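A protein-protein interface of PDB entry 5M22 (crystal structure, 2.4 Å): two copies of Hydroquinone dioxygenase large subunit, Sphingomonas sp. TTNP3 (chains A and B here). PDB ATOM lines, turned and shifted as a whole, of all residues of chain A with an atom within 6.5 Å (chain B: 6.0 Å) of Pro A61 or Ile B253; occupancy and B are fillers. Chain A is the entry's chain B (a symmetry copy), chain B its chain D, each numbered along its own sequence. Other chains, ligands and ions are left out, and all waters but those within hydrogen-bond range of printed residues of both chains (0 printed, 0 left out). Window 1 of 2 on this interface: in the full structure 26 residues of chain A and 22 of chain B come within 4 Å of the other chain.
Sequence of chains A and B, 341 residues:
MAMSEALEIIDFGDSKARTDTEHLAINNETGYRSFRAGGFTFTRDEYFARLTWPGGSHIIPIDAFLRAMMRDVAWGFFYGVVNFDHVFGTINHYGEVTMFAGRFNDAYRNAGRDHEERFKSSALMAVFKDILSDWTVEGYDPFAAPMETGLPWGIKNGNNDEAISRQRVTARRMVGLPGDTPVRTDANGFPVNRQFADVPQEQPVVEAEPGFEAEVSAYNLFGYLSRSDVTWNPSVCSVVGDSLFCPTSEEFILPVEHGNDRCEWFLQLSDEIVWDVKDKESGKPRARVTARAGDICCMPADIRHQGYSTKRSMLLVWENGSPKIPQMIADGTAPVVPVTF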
ATOM      1  N   TYR A  47     -27.868   9.250  -2.770  1.00  0.00           N
ATOM      2  CA  TYR A  47     -26.616   9.376  -3.515  1.00  0.00           C
ATOM      3  C   TYR A  47     -25.505  10.037  -2.718  1.00  0.00           C
ATOM      4  O   TYR A  47     -24.332   9.942  -3.109  1.00  0.00           O
ATOM      5  CB  TYR A  47     -26.814  10.235  -4.783  1.00  0.00           C
ATOM      6  CG  TYR A  47     -27.374   9.527  -5.991  1.00  0.00           C
ATOM      7  CD1 TYR A  47     -26.749   8.411  -6.515  1.00  0.00           C
ATOM      8  CD2 TYR A  47     -28.527  10.007  -6.639  1.00  0.00           C
ATOM      9  CE1 TYR A  47     -27.260   7.743  -7.641  1.00  0.00           C
ATOM     10  CE2 TYR A  47     -29.060   9.365  -7.768  1.00  0.00           C
ATOM     11  CZ  TYR A  47     -28.409   8.228  -8.286  1.00  0.00           C
ATOM     12  OH  TYR A  47     -28.903   7.556  -9.402  1.00  0.00           O
ATOM     13  N   PHE A  48     -25.872  10.738  -1.635  1.00  0.00           N
ATOM     14  CA  PHE A  48     -24.992  11.778  -1.050  1.00  0.00           C
ATOM     15  C   PHE A  48     -24.924  11.803   0.456  1.00  0.00           C
ATOM     16  O   PHE A  48     -25.941  11.646   1.157  1.00  0.00           O
ATOM     17  CB  PHE A  48     -25.385  13.195  -1.509  1.00  0.00           C
ATOM     18  CG  PHE A  48     -25.256  13.418  -2.983  1.00  0.00           C
ATOM     19  CD1 PHE A  48     -24.035  13.167  -3.653  1.00  0.00           C
ATOM     20  CD2 PHE A  48     -26.336  13.876  -3.720  1.00  0.00           C
ATOM     21  CE1 PHE A  48     -23.920  13.366  -5.016  1.00  0.00           C
ATOM     22  CE2 PHE A  48     -26.215  14.072  -5.091  1.00  0.00           C
ATOM     23  CZ  PHE A  48     -25.007  13.817  -5.741  1.00  0.00           C
ATOM     24  N   ALA A  49     -23.723  12.068   0.951  1.00  0.00           N
ATOM     25  CA  ALA A  49     -23.568  12.464   2.328  1.00  0.00           C
ATOM     26  C   ALA A  49     -23.573  13.965   2.303  1.00  0.00           C
ATOM     27  O   ALA A  49     -22.846  14.574   1.512  1.00  0.00           O
ATOM     28  CB  ALA A  49     -22.266  11.931   2.884  1.00  0.00           C
ATOM     29  N   ILE A  59     -20.816  18.376   0.041  1.00  0.00           N
ATOM     30  CA  ILE A  59     -21.433  17.100  -0.319  1.00  0.00           C
ATOM     31  C   ILE A  59     -20.335  16.147  -0.737  1.00  0.00           C
ATOM     32  O   ILE A  59     -19.333  16.582  -1.287  1.00  0.00           O
ATOM     33  CB  ILE A  59     -22.470  17.273  -1.452  1.00  0.00           C
ATOM     34  CG1 ILE A  59     -23.651  18.120  -0.975  1.00  0.00           C
ATOM     35  CG2 ILE A  59     -22.998  15.924  -1.938  1.00  0.00           C
ATOM     36  CD1 ILE A  59     -24.543  18.636  -2.089  1.00  0.00           C
ATOM     37  N   ILE A  60     -20.527  14.857  -0.465  1.00  0.00           N
ATOM     38  CA  ILE A  60     -19.577  13.805  -0.842  1.00  0.00           C
ATOM     39  C   ILE A  60     -20.432  12.632  -1.261  1.00  0.00           C
ATOM     40  O   ILE A  60     -21.411  12.322  -0.596  1.00  0.00           O
ATOM     41  CB  ILE A  60     -18.663  13.396   0.360  1.00  0.00           C
ATOM     42  CG1 ILE A  60     -17.748  14.566   0.758  1.00  0.00           C
ATOM     43  CG2 ILE A  60     -17.862  12.142   0.057  1.00  0.00           C
ATOM     44  CD1 ILE A  60     -17.023  14.384   2.096  1.00  0.00           C
ATOM     45  N   PRO A  61     -20.084  11.993  -2.381  1.00  0.00           N
ATOM     46  CA  PRO A  61     -20.753  10.784  -2.825  1.00  0.00           C
ATOM     47  C   PRO A  61     -20.833   9.804  -1.680  1.00  0.00           C
ATOM     48  O   PRO A  61     -19.830   9.590  -0.960  1.00  0.00           O
ATOM     49  CB  PRO A  61     -19.812  10.250  -3.906  1.00  0.00           C
ATOM     50  CG  PRO A  61     -19.198  11.470  -4.470  1.00  0.00           C
ATOM     51  CD  PRO A  61     -19.043  12.422  -3.335  1.00  0.00           C
ATOM     52  N   ILE A  62     -22.006   9.227  -1.492  1.00  0.00           N
ATOM     53  CA  ILE A  62     -22.199   8.364  -0.332  1.00  0.00           C
ATOM     54  C   ILE A  62     -21.211   7.170  -0.286  1.00  0.00           C
ATOM     55  O   ILE A  62     -20.842   6.702   0.808  1.00  0.00           O
ATOM     56  CB  ILE A  62     -23.679   7.910  -0.149  1.00  0.00           C
ATOM     57  CG1 ILE A  62     -23.906   7.477   1.311  1.00  0.00           C
ATOM     58  CG2 ILE A  62     -24.072   6.792  -1.122  1.00  0.00           C
ATOM     59  CD1 ILE A  62     -23.324   8.428   2.342  1.00  0.00           C
ATOM     60  N   ASP A  63     -20.773   6.686  -1.447  1.00  0.00           N
ATOM     61  CA  ASP A  63     -19.878   5.530  -1.440  1.00  0.00           C
ATOM     62  C   ASP A  63     -18.489   5.944  -1.002  1.00  0.00           C
ATOM     63  O   ASP A  63     -17.915   5.303  -0.109  1.00  0.00           O
ATOM     64  CB  ASP A  63     -19.818   4.818  -2.783  1.00  0.00           C
ATOM     65  CG  ASP A  63     -19.446   5.760  -3.950  1.00  0.00           C
ATOM     66  OD1 ASP A  63     -19.534   7.022  -3.861  1.00  0.00           O
ATOM     67  OD2 ASP A  63     -19.095   5.180  -4.989  1.00  0.00           O
ATOM     68  N   ALA A  64     -17.970   7.025  -1.591  1.00  0.00           N
ATOM     69  CA  ALA A  64     -16.693   7.559  -1.152  1.00  0.00           C
ATOM     70  C   ALA A  64     -16.746   7.898   0.328  1.00  0.00           C
ATOM     71  O   ALA A  64     -15.810   7.592   1.025  1.00  0.00           O
ATOM     72  CB  ALA A  64     -16.273   8.753  -1.979  1.00  0.00           C
ATOM     73  N   PHE A  65     -17.828   8.507   0.825  1.00  0.00           N
ATOM     74  CA  PHE A  65     -17.948   8.836   2.266  1.00  0.00           C
ATOM     75  C   PHE A  65     -17.875   7.630   3.188  1.00  0.00           C
ATOM     76  O   PHE A  65     -17.104   7.613   4.133  1.00  0.00           O
ATOM     77  CB  PHE A  65     -19.266   9.549   2.539  1.00  0.00           C
ATOM     78  CG  PHE A  65     -19.370  10.146   3.917  1.00  0.00           C
ATOM     79  CD1 PHE A  65     -18.860  11.412   4.180  1.00  0.00           C
ATOM     80  CD2 PHE A  65     -20.004   9.456   4.948  1.00  0.00           C
ATOM     81  CE1 PHE A  65     -18.947  11.972   5.455  1.00  0.00           C
ATOM     82  CE2 PHE A  65     -20.100  10.004   6.230  1.00  0.00           C
ATOM     83  CZ  PHE A  65     -19.564  11.274   6.482  1.00  0.00           C
ATOM     84  N   LEU A  66     -18.693   6.613   2.930  1.00  0.00           N
ATOM     85  CA  LEU A  66     -18.734   5.459   3.810  1.00  0.00           C
ATOM     86  C   LEU A  66     -17.393   4.733   3.866  1.00  0.00           C
ATOM     87  O   LEU A  66     -17.008   4.253   4.948  1.00  0.00           O
ATOM     88  CB  LEU A  66     -19.863   4.514   3.425  1.00  0.00           C
ATOM     89  CG  LEU A  66     -21.281   5.060   3.626  1.00  0.00           C
ATOM     90  CD1 LEU A  66     -22.291   4.269   2.810  1.00  0.00           C
ATOM     91  CD2 LEU A  66     -21.690   5.071   5.081  1.00  0.00           C
ATOM     92  N   TRP A 153     -26.344   2.886  -2.955  1.00  0.00           N
ATOM     93  CA  TRP A 153     -27.393   3.777  -3.475  1.00  0.00           C
ATOM     94  C   TRP A 153     -28.796   3.468  -2.950  1.00  0.00           C
ATOM     95  O   TRP A 153     -29.060   2.365  -2.523  1.00  0.00           O
ATOM     96  CB  TRP A 153     -27.413   3.701  -5.006  1.00  0.00           C
ATOM     97  CG  TRP A 153     -26.057   3.777  -5.662  1.00  0.00           C
ATOM     98  CD1 TRP A 153     -25.537   2.910  -6.600  1.00  0.00           C
ATOM     99  CD2 TRP A 153     -25.048   4.786  -5.440  1.00  0.00           C
ATOM    100  NE1 TRP A 153     -24.264   3.345  -6.992  1.00  0.00           N
ATOM    101  CE2 TRP A 153     -23.949   4.483  -6.293  1.00  0.00           C
ATOM    102  CE3 TRP A 153     -24.989   5.938  -4.641  1.00  0.00           C
ATOM    103  CZ2 TRP A 153     -22.796   5.290  -6.348  1.00  0.00           C
ATOM    104  CZ3 TRP A 153     -23.834   6.732  -4.678  1.00  0.00           C
ATOM    105  CH2 TRP A 153     -22.753   6.405  -5.530  1.00  0.00           C
ATOM    106  N   ARG B  67     -18.041   8.585 -17.916  1.00  0.00           N
ATOM    107  CA  ARG B  67     -19.100   9.609 -17.791  1.00  0.00           C
ATOM    108  C   ARG B  67     -18.691  10.963 -18.375  1.00  0.00           C
ATOM    109  O   ARG B  67     -19.465  11.583 -19.129  1.00  0.00           O
ATOM    110  CB  ARG B  67     -19.529   9.752 -16.329  1.00  0.00           C
ATOM    111  CG  ARG B  67     -20.243   8.501 -15.895  1.00  0.00           C
ATOM    112  CD  ARG B  67     -21.140   8.670 -14.687  1.00  0.00           C
ATOM    113  NE  ARG B  67     -20.445   8.161 -13.525  1.00  0.00           N
ATOM    114  CZ  ARG B  67     -19.771   8.952 -12.720  1.00  0.00           C
ATOM    115  NH1 ARG B  67     -19.774  10.263 -12.976  1.00  0.00           N
ATOM    116  NH2 ARG B  67     -19.130   8.452 -11.670  1.00  0.00           N
ATOM    117  N   TRP B 232     -27.726  15.145 -17.712  1.00  0.00           N
ATOM    118  CA  TRP B 232     -26.788  16.215 -17.970  1.00  0.00           C
ATOM    119  C   TRP B 232     -26.487  16.434 -19.458  1.00  0.00           C
ATOM    120  O   TRP B 232     -25.340  16.424 -19.849  1.00  0.00           O
ATOM    121  CB  TRP B 232     -25.500  15.923 -17.197  1.00  0.00           C
ATOM    122  CG  TRP B 232     -25.722  15.784 -15.730  1.00  0.00           C
ATOM    123  CD1 TRP B 232     -25.743  14.628 -15.025  1.00  0.00           C
ATOM    124  CD2 TRP B 232     -25.951  16.846 -14.794  1.00  0.00           C
ATOM    125  NE1 TRP B 232     -25.968  14.897 -13.687  1.00  0.00           N
ATOM    126  CE2 TRP B 232     -26.101  16.255 -13.521  1.00  0.00           C
ATOM    127  CE3 TRP B 232     -26.030  18.246 -14.905  1.00  0.00           C
ATOM    128  CZ2 TRP B 232     -26.322  17.024 -12.343  1.00  0.00           C
ATOM    129  CZ3 TRP B 232     -26.278  19.008 -13.747  1.00  0.00           C
ATOM    130  CH2 TRP B 232     -26.411  18.395 -12.490  1.00  0.00           C
ATOM    131  N   GLU B 251     -29.409  14.227 -12.840  1.00  0.00           N
ATOM    132  CA  GLU B 251     -29.364  13.272 -11.745  1.00  0.00           C
ATOM    133  C   GLU B 251     -27.930  12.897 -11.336  1.00  0.00           C
ATOM    134  O   GLU B 251     -27.098  12.615 -12.178  1.00  0.00           O
ATOM    135  CB  GLU B 251     -30.158  12.014 -12.116  1.00  0.00           C
ATOM    136  CG  GLU B 251     -30.543  11.160 -10.909  1.00  0.00           C
ATOM    137  CD  GLU B 251     -31.241   9.863 -11.294  1.00  0.00           C
ATOM    138  OE1 GLU B 251     -31.896   9.808 -12.373  1.00  0.00           O
ATOM    139  OE2 GLU B 251     -31.108   8.891 -10.520  1.00  0.00           O
ATOM    140  N   PHE B 252     -27.679  12.845 -10.024  1.00  0.00           N
ATOM    141  CA  PHE B 252     -26.370  12.546  -9.469  1.00  0.00           C
ATOM    142  C   PHE B 252     -25.463  13.782  -9.603  1.00  0.00           C
ATOM    143  O   PHE B 252     -25.866  14.875  -9.181  1.00  0.00           O
ATOM    144  CB  PHE B 252     -25.752  11.275 -10.100  1.00  0.00           C
ATOM    145  CG  PHE B 252     -24.562  10.723  -9.330  1.00  0.00           C
ATOM    146  CD1 PHE B 252     -24.656  10.449  -7.973  1.00  0.00           C
ATOM    147  CD2 PHE B 252     -23.334  10.502  -9.962  1.00  0.00           C
ATOM    148  CE1 PHE B 252     -23.561   9.965  -7.254  1.00  0.00           C
ATOM    149  CE2 PHE B 252     -22.239  10.021  -9.245  1.00  0.00           C
ATOM    150  CZ  PHE B 252     -22.353   9.745  -7.885  1.00  0.00           C
ATOM    151  N   ILE B 253     -24.272  13.618 -10.192  1.00  0.00           N
ATOM    152  CA  ILE B 253     -23.272  14.678 -10.309  1.00  0.00           C
ATOM    153  C   ILE B 253     -22.959  14.982 -11.771  1.00  0.00           C
ATOM    154  O   ILE B 253     -22.708  14.065 -12.524  1.00  0.00           O
ATOM    155  CB  ILE B 253     -21.941  14.242  -9.652  1.00  0.00           C
ATOM    156  CG1 ILE B 253     -22.184  13.718  -8.239  1.00  0.00           C
ATOM    157  CG2 ILE B 253     -20.929  15.382  -9.689  1.00  0.00           C
ATOM    158  CD1 ILE B 253     -20.914  13.329  -7.507  1.00  0.00           C
ATOM    159  N   LEU B 254     -22.982  16.245 -12.184  1.00  0.00           N
ATOM    160  CA  LEU B 254     -22.519  16.591 -13.543  1.00  0.00           C
ATOM    161  C   LEU B 254     -21.102  16.044 -13.652  1.00  0.00           C
ATOM    162  O   LEU B 254     -20.284  16.383 -12.820  1.00  0.00           O
ATOM    163  CB  LEU B 254     -22.531  18.113 -13.753  1.00  0.00           C
ATOM    164  CG  LEU B 254     -21.861  18.744 -14.966  1.00  0.00           C
ATOM    165  CD1 LEU B 254     -22.628  18.450 -16.229  1.00  0.00           C
ATOM    166  CD2 LEU B 254     -21.752  20.249 -14.792  1.00  0.00           C
ATOM    167  N   PRO B 255     -20.819  15.163 -14.651  1.00  0.00           N
ATOM    168  CA  PRO B 255     -19.555  14.408 -14.774  1.00  0.00           C
ATOM    169  C   PRO B 255     -18.301  15.208 -15.080  1.00  0.00           C
ATOM    170  O   PRO B 255     -17.236  14.611 -15.213  1.00  0.00           O
ATOM    171  CB  PRO B 255     -19.807  13.476 -15.951  1.00  0.00           C
ATOM    172  CG  PRO B 255     -21.306  13.391 -16.084  1.00  0.00           C
ATOM    173  CD  PRO B 255     -21.790  14.757 -15.692  1.00  0.00           C
ATOM    174  N   VAL B 256     -18.405  16.530 -15.195  1.00  0.00           N
ATOM    175  CA  VAL B 256     -17.265  17.380 -15.508  1.00  0.00           C
ATOM    176  C   VAL B 256     -17.435  18.683 -14.743  1.00  0.00           C
ATOM    177  O   VAL B 256     -18.516  18.942 -14.217  1.00  0.00           O
ATOM    178  CB  VAL B 256     -17.178  17.702 -17.018  1.00  0.00           C
ATOM    179  CG1 VAL B 256     -17.265  16.433 -17.881  1.00  0.00           C
ATOM    180  CG2 VAL B 256     -18.249  18.715 -17.424  1.00  0.00           C
ATOM    181  N   GLN B 306     -19.901  22.633 -11.192  1.00  0.00           N
ATOM    182  CA  GLN B 306     -20.229  21.220 -11.147  1.00  0.00           C
ATOM    183  C   GLN B 306     -21.508  21.019 -10.311  1.00  0.00           C
ATOM    184  O   GLN B 306     -21.538  21.392  -9.147  1.00  0.00           O
ATOM    185  CB  GLN B 306     -19.033  20.411 -10.599  1.00  0.00           C
ATOM    186  CG  GLN B 306     -19.284  18.908 -10.585  1.00  0.00           C
ATOM    187  CD  GLN B 306     -18.042  18.060 -10.508  1.00  0.00           C
ATOM    188  OE1 GLN B 306     -17.216  18.224  -9.618  1.00  0.00           O
ATOM    189  NE2 GLN B 306     -17.920  17.119 -11.433  1.00  0.00           N
ATOM    190  N   GLY B 307     -22.561  20.443 -10.895  1.00  0.00           N
ATOM    191  CA  GLY B 307     -23.869  20.321 -10.206  1.00  0.00           C
ATOM    192  C   GLY B 307     -24.186  19.051  -9.428  1.00  0.00           C
ATOM    193  O   GLY B 307     -23.807  17.950  -9.820  1.00  0.00           O
ATOM    194  N   TYR B 308     -24.878  19.195  -8.313  1.00  0.00           N
ATOM    195  CA  TYR B 308     -25.358  18.024  -7.563  1.00  0.00           C
ATOM    196  C   TYR B 308     -26.884  17.959  -7.530  1.00  0.00           C
ATOM    197  O   TYR B 308     -27.514  18.870  -7.014  1.00  0.00           O
ATOM    198  CB  TYR B 308     -24.817  18.059  -6.150  1.00  0.00           C
ATOM    199  CG  TYR B 308     -23.331  17.895  -6.156  1.00  0.00           C
ATOM    200  CD1 TYR B 308     -22.505  18.960  -6.457  1.00  0.00           C
ATOM    201  CD2 TYR B 308     -22.753  16.649  -5.917  1.00  0.00           C
ATOM    202  CE1 TYR B 308     -21.131  18.800  -6.508  1.00  0.00           C
ATOM    203  CE2 TYR B 308     -21.376  16.484  -5.935  1.00  0.00           C
ATOM    204  CZ  TYR B 308     -20.575  17.567  -6.253  1.00  0.00           C
ATOM    205  OH  TYR B 308     -19.211  17.434  -6.290  1.00  0.00           O
ATOM    206  N   SER B 309     -27.457  16.894  -8.101  1.00  0.00           N
ATOM    207  CA  SER B 309     -28.903  16.666  -8.090  1.00  0.00           C
ATOM    208  C   SER B 309     -29.281  15.296  -7.493  1.00  0.00           C
ATOM    209  O   SER B 309     -29.123  14.244  -8.138  1.00  0.00           O
ATOM    210  CB  SER B 309     -29.441  16.809  -9.518  1.00  0.00           C
ATOM    211  OG  SER B 309     -30.844  16.941  -9.520  1.00  0.00           O
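OE2 of Glu B251 sits at hydrogen-bond distance from OH of Tyr A47 (2.8 Å).
The backbone carbonyl oxygen (O) of Glu B251 sits at hydrogen-bond distance from the indole nitrogen (NE1) of Trp B232, 3.0 Å away. The backbone NH (N) of Phe B252 sits at hydrogen-bond distance from the backbone carbonyl oxygen (O) of Ser B309 (2.8 Å). O of Tyr A47 is in hydrogen-bond range of N of Ile A62.
CD1 of Phe B252 touches CD1 of Tyr A47, 3.3 Å away. Phe A48 touches Phe B252. Phe A48 touches Ile B253. Tyr B308 touches Phe A48. Pro A61 touches Ile B253 (CG to CD1, 3.95 Å).
Of the printed residues of chain B, Tyr A47 touches Glu B251 and Phe B252. Of the printed residues of chain B, Phe A48 touches Phe B252 (3.7 Å), Ile B253 (3.7 Å) and Tyr B308 (3.6 Å). Of chain B, only Ile B253 comes within 4 Å of Pro A61. Printed residues of chain A within 4 Å of Glu B251: Tyr A47. Of the printed residues of chain A, Phe B252 touches Tyr A47 and Phe A48. Of chain A, only Phe A48 (3.7 Å) and Pro A61 (3.95 Å) come within 4 Å of Ile B253. Printed residues of chain A within 4 Å of Tyr B308: Phe A48 (3.6 Å). The nearest residue of chain A that does not touch Ile B253 is Ile A60 (6.3 Å). The nearest printed residue of chain A that does not touch Phe B252 is Trp A153 (4.04 Å).
Of the 12 printed residues of chain B, 4 touch a printed residue of chain A. Printed residues of chain B that touch a printed residue of chain A: Glu B251, Phe B252, Ile B253 and Tyr B308. Hydrophobic or aromatic side chains of chain B within 4 Å of the printed part of chain A: Phe B252, Ile B253 and Tyr B308. Among the printed residues, no Asp or Glu carboxylate lies within 4 Å of a Lys or Arg side-chain nitrogen of the other chain.
No position is printed for both chains.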
